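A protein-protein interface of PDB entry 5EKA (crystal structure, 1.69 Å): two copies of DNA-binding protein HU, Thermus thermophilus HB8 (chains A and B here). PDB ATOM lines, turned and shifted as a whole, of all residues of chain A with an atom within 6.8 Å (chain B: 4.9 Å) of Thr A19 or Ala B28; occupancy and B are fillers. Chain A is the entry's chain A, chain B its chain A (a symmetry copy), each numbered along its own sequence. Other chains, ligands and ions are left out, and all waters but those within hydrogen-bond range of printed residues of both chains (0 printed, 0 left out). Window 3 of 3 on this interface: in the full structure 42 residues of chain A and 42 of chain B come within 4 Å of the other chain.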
ATOM      1  N   GLN A  14      18.273  11.659 -25.235  1.00  0.00           N
ATOM      2  CA  GLN A  14      18.037  11.453 -23.817  1.00  0.00           C
ATOM      3  C   GLN A  14      17.769  12.777 -23.121  1.00  0.00           C
ATOM      4  O   GLN A  14      16.890  12.869 -22.313  1.00  0.00           O
ATOM      5  CB  GLN A  14      19.251  10.795 -23.173  1.00  0.00           C
ATOM      6  CG  GLN A  14      19.421   9.343 -23.568  1.00  0.00           C
ATOM      7  CD  GLN A  14      20.667   8.709 -23.014  1.00  0.00           C
ATOM      8  OE1 GLN A  14      21.311   9.254 -22.170  1.00  0.00           O
ATOM      9  NE2 GLN A  14      21.033   7.535 -23.557  1.00  0.00           N
ATOM     10  N   VAL A  15      18.525  13.800 -23.483  1.00  0.00           N
ATOM     11  CA  VAL A  15      18.349  15.124 -22.886  1.00  0.00           C
ATOM     12  C   VAL A  15      17.036  15.781 -23.335  1.00  0.00           C
ATOM     13  O   VAL A  15      16.327  16.378 -22.520  1.00  0.00           O
ATOM     14  CB  VAL A  15      19.553  16.074 -23.159  1.00  0.00           C
ATOM     15  CG1 VAL A  15      19.242  17.466 -22.607  1.00  0.00           C
ATOM     16  CG2 VAL A  15      20.851  15.576 -22.537  1.00  0.00           C
ATOM     17  N   ALA A  16      16.696  15.692 -24.620  1.00  0.00           N
ATOM     18  CA  ALA A  16      15.388  16.180 -25.086  1.00  0.00           C
ATOM     19  C   ALA A  16      14.252  15.560 -24.281  1.00  0.00           C
ATOM     20  O   ALA A  16      13.339  16.240 -23.801  1.00  0.00           O
ATOM     21  CB  ALA A  16      15.212  15.906 -26.576  1.00  0.00           C
ATOM     22  N   GLN A  17      14.320  14.257 -24.115  1.00  0.00           N
ATOM     23  CA  GLN A  17      13.340  13.556 -23.351  1.00  0.00           C
ATOM     24  C   GLN A  17      13.256  13.996 -21.886  1.00  0.00           C
ATOM     25  O   GLN A  17      12.142  14.181 -21.373  1.00  0.00           O
ATOM     26  CB  GLN A  17      13.614  12.073 -23.442  1.00  0.00           C
ATOM     27  CG  GLN A  17      12.581  11.224 -22.785  1.00  0.00           C
ATOM     28  CD  GLN A  17      12.641   9.805 -23.296  1.00  0.00           C
ATOM     29  OE1 GLN A  17      13.521   9.034 -22.895  1.00  0.00           O
ATOM     30  NE2 GLN A  17      11.720   9.451 -24.210  1.00  0.00           N
ATOM     31  N   ALA A  18      14.397  14.120 -21.214  1.00  0.00           N
ATOM     32  CA  ALA A  18      14.437  14.440 -19.790  1.00  0.00           C
ATOM     33  C   ALA A  18      13.970  15.877 -19.504  1.00  0.00           C
ATOM     34  O   ALA A  18      13.319  16.123 -18.488  1.00  0.00           O
ATOM     35  CB  ALA A  18      15.845  14.213 -19.244  1.00  0.00           C
ATOM     36  N   THR A  19      14.257  16.794 -20.423  1.00  0.00           N
ATOM     37  CA  THR A  19      13.978  18.224 -20.234  1.00  0.00           C
ATOM     38  C   THR A  19      12.665  18.674 -20.872  1.00  0.00           C
ATOM     39  O   THR A  19      12.162  19.781 -20.575  1.00  0.00           O
ATOM     40  CB  THR A  19      15.079  19.104 -20.851  1.00  0.00           C
ATOM     41  OG1 THR A  19      15.183  18.860 -22.267  1.00  0.00           O
ATOM     42  CG2 THR A  19      16.378  18.851 -20.170  1.00  0.00           C
ATOM     43  N   GLY A  20      12.145  17.860 -21.789  1.00  0.00           N
ATOM     44  CA  GLY A  20      11.001  18.243 -22.600  1.00  0.00           C
ATOM     45  C   GLY A  20      11.280  19.354 -23.591  1.00  0.00           C
ATOM     46  O   GLY A  20      10.348  19.995 -24.068  1.00  0.00           O
ATOM     47  N   LEU A  21      12.557  19.606 -23.888  1.00  0.00           N
ATOM     48  CA  LEU A  21      12.934  20.624 -24.856  1.00  0.00           C
ATOM     49  C   LEU A  21      13.049  20.002 -26.241  1.00  0.00           C
ATOM     50  O   LEU A  21      13.147  18.787 -26.372  1.00  0.00           O
ATOM     51  CB  LEU A  21      14.203  21.344 -24.421  1.00  0.00           C
ATOM     52  CG  LEU A  21      14.024  22.078 -23.074  1.00  0.00           C
ATOM     53  CD1 LEU A  21      15.362  22.352 -22.391  1.00  0.00           C
ATOM     54  CD2 LEU A  21      13.191  23.355 -23.236  1.00  0.00           C
ATOM     55  N   LYS A  22      12.959  20.839 -27.270  1.00  0.00           N
ATOM     56  CA  LYS A  22      12.995  20.367 -28.653  1.00  0.00           C
ATOM     57  C   LYS A  22      14.343  19.773 -29.005  1.00  0.00           C
ATOM     58  O   LYS A  22      15.385  20.325 -28.657  1.00  0.00           O
ATOM     59  CB  LYS A  22      12.689  21.496 -29.633  1.00  0.00           C
ATOM     60  CG  LYS A  22      11.320  22.113 -29.479  1.00  0.00           C
ATOM     61  CD  LYS A  22      11.139  23.222 -30.505  1.00  0.00           C
ATOM     62  CE  LYS A  22      10.633  24.509 -29.873  1.00  0.00           C
ATOM     63  NZ  LYS A  22      11.685  25.140 -29.019  1.00  0.00           N
ATOM     64  N   VAL A  26      18.184  21.127 -28.441  1.00  0.00           N
ATOM     65  CA  VAL A  26      19.184  20.393 -27.634  1.00  0.00           C
ATOM     66  C   VAL A  26      20.394  20.127 -28.521  1.00  0.00           C
ATOM     67  O   VAL A  26      21.512  20.252 -28.104  1.00  0.00           O
ATOM     68  CB  VAL A  26      18.596  19.060 -27.080  1.00  0.00           C
ATOM     69  CG1 VAL A  26      19.652  18.261 -26.364  1.00  0.00           C
ATOM     70  CG2 VAL A  26      17.398  19.346 -26.150  1.00  0.00           C
ATOM     71  N   LYS B  24      17.574  29.821 -19.063  1.00  0.00           N
ATOM     72  CA  LYS B  24      16.903  28.806 -18.237  1.00  0.00           C
ATOM     73  C   LYS B  24      16.895  27.426 -18.929  1.00  0.00           C
ATOM     74  O   LYS B  24      17.009  26.390 -18.271  1.00  0.00           O
ATOM     75  CB  LYS B  24      15.460  29.232 -17.868  1.00  0.00           C
ATOM     76  CG  LYS B  24      14.410  28.950 -18.948  1.00  0.00           C
ATOM     77  CD  LYS B  24      13.026  29.458 -18.589  1.00  0.00           C
ATOM     78  CE  LYS B  24      11.961  28.770 -19.448  1.00  0.00           C
ATOM     79  NZ  LYS B  24      10.688  29.548 -19.574  1.00  0.00           N
ATOM     80  N   ASP B  25      16.755  27.434 -20.253  1.00  0.00           N
ATOM     81  CA  ASP B  25      16.677  26.205 -21.039  1.00  0.00           C
ATOM     82  C   ASP B  25      18.056  25.613 -21.199  1.00  0.00           C
ATOM     83  O   ASP B  25      18.223  24.414 -21.069  1.00  0.00           O
ATOM     84  CB  ASP B  25      16.031  26.453 -22.424  1.00  0.00           C
ATOM     85  CG  ASP B  25      14.496  26.693 -22.355  1.00  0.00           C
ATOM     86  OD1 ASP B  25      13.852  26.446 -21.304  1.00  0.00           O
ATOM     87  OD2 ASP B  25      13.909  27.119 -23.380  1.00  0.00           O
ATOM     88  N   VAL B  26      19.045  26.455 -21.452  1.00  0.00           N
ATOM     89  CA  VAL B  26      20.433  25.971 -21.625  1.00  0.00           C
ATOM     90  C   VAL B  26      20.892  25.386 -20.295  1.00  0.00           C
ATOM     91  O   VAL B  26      21.525  24.367 -20.247  1.00  0.00           O
ATOM     92  CB  VAL B  26      21.380  27.121 -22.083  1.00  0.00           C
ATOM     93  CG1 VAL B  26      22.810  26.652 -22.139  1.00  0.00           C
ATOM     94  CG2 VAL B  26      20.930  27.676 -23.451  1.00  0.00           C
ATOM     95  N   LYS B  27      20.518  26.032 -19.188  1.00  0.00           N
ATOM     96  CA  LYS B  27      20.938  25.535 -17.877  1.00  0.00           C
ATOM     97  C   LYS B  27      20.385  24.132 -17.570  1.00  0.00           C
ATOM     98  O   LYS B  27      21.124  23.240 -17.079  1.00  0.00           O
ATOM     99  CB  LYS B  27      20.534  26.556 -16.805  1.00  0.00           C
ATOM    100  CG  LYS B  27      20.563  26.023 -15.392  1.00  0.00           C
ATOM    101  CD  LYS B  27      21.926  25.633 -14.920  1.00  0.00           C
ATOM    102  CE  LYS B  27      21.917  25.290 -13.429  1.00  0.00           C
ATOM    103  NZ  LYS B  27      23.111  24.483 -13.035  1.00  0.00           N
ATOM    104  N   ALA B  28      19.130  23.920 -17.943  1.00  0.00           N
ATOM    105  CA  ALA B  28      18.436  22.644 -17.772  1.00  0.00           C
ATOM    106  C   ALA B  28      19.082  21.595 -18.669  1.00  0.00           C
ATOM    107  O   ALA B  28      19.238  20.438 -18.269  1.00  0.00           O
ATOM    108  CB  ALA B  28      16.960  22.812 -18.117  1.00  0.00           C
ATOM    109  N   MET B  29      19.438  21.992 -19.881  1.00  0.00           N
ATOM    110  CA  MET B  29      20.066  21.066 -20.829  1.00  0.00           C
ATOM    111  C   MET B  29      21.437  20.583 -20.366  1.00  0.00           C
ATOM    112  O   MET B  29      21.716  19.373 -20.406  1.00  0.00           O
ATOM    113  CB  MET B  29      20.117  21.689 -22.226  1.00  0.00           C
ATOM    114  CG  MET B  29      18.758  21.851 -22.873  1.00  0.00           C
ATOM    115  SD  MET B  29      19.010  22.625 -24.481  1.00  0.00           S
ATOM    116  CE  MET B  29      17.316  22.844 -24.983  1.00  0.00           C
ATOM    117  N   VAL B  30      22.270  21.513 -19.882  1.00  0.00           N
ATOM    118  CA  VAL B  30      23.604  21.184 -19.419  1.00  0.00           C
ATOM    119  C   VAL B  30      23.523  20.258 -18.209  1.00  0.00           C
ATOM    120  O   VAL B  30      24.234  19.262 -18.148  1.00  0.00           O
ATOM    121  CB  VAL B  30      24.512  22.409 -19.115  1.00  0.00           C
ATOM    122  CG1 VAL B  30      25.874  21.952 -18.603  1.00  0.00           C
ATOM    123  CG2 VAL B  30      24.707  23.278 -20.353  1.00  0.00           C
ATOM    124  N   ASP B  31      22.632  20.556 -17.268  1.00  0.00           N
ATOM    125  CA  ASP B  31      22.561  19.699 -16.080  1.00  0.00           C
ATOM    126  C   ASP B  31      22.096  18.292 -16.473  1.00  0.00           C
ATOM    127  O   ASP B  31      22.634  17.302 -15.996  1.00  0.00           O
ATOM    128  CB  ASP B  31      21.625  20.302 -15.030  1.00  0.00           C
ATOM    129  CG  ASP B  31      22.239  21.520 -14.344  1.00  0.00           C
ATOM    130  OD1 ASP B  31      23.471  21.705 -14.456  1.00  0.00           O
ATOM    131  OD2 ASP B  31      21.474  22.247 -13.668  1.00  0.00           O
ATOM    132  N   ALA B  32      21.115  18.220 -17.372  1.00  0.00           N
ATOM    133  CA  ALA B  32      20.636  16.918 -17.855  1.00  0.00           C
ATOM    134  C   ALA B  32      21.724  16.182 -18.619  1.00  0.00           C
ATOM    135  O   ALA B  32      21.865  14.980 -18.485  1.00  0.00           O
ATOM    136  CB  ALA B  32      19.387  17.055 -18.721  1.00  0.00           C
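1 position is printed for both chains.
Of the 7 pairs that touch across the chains among the printed residues, none has its exchanged pair printed and touching as well.
O of Val A15 lies within hydrogen-bond range of OG1 of Thr A19, at 2.7 Å.
The backbone carbonyl oxygen (O) of Ala A16 is in hydrogen-bond range of the backbone NH (N) of Leu A21 (3.5 Å).
OG1 of Thr A19 lies close to N of Leu A21.
Printed residues of chain B within 4 Å of Thr A19: Ala B28 (3.8 Å) and Ala B32 (3.8 Å).
Of chain A, only Thr A19 comes within 4 Å of Ala B28.
Printed residues of chain B within 4 Å of Val A15: Met B29 and Ala B32.
Of the printed residues of chain A, Met B29 touches Val A15, Leu A21 and Val A26.
Printed residues of chain A within 4 Å of Asp B25: Leu A21 (3.7 Å).
Of the printed residues of chain B, Val A26 touches Met B29.
The nearest residue of chain B that does not touch Thr A19 is Met B29 (4.4 Å).
The nearest printed residue of chain B that does not touch Val A15 is Ala B28 (5.3 Å).
O of Met B29 touches CG1 of Val A15, at 3.8 Å.
CB of Ala B32 touches CG1 of Val A15, 3.9 Å away.
Ala B28 touches Thr A19.
Ala B32 touches Thr A19.
Asp B25 touches Leu A21.
Met B29 touches Leu A21.
Val A26 touches Met B29 (CG2 to CE, 3.7 Å).
Of the 9 printed residues of chain B, 4 touch a printed residue of chain A.
Hydrophobic or aromatic side chains of chain B that line the printed part of chain A: Met B29 and Ala B32.
Among the printed residues, no Asp or Glu carboxylate lies within 4 Å of a Lys or Arg side-chain nitrogen of the other chain.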
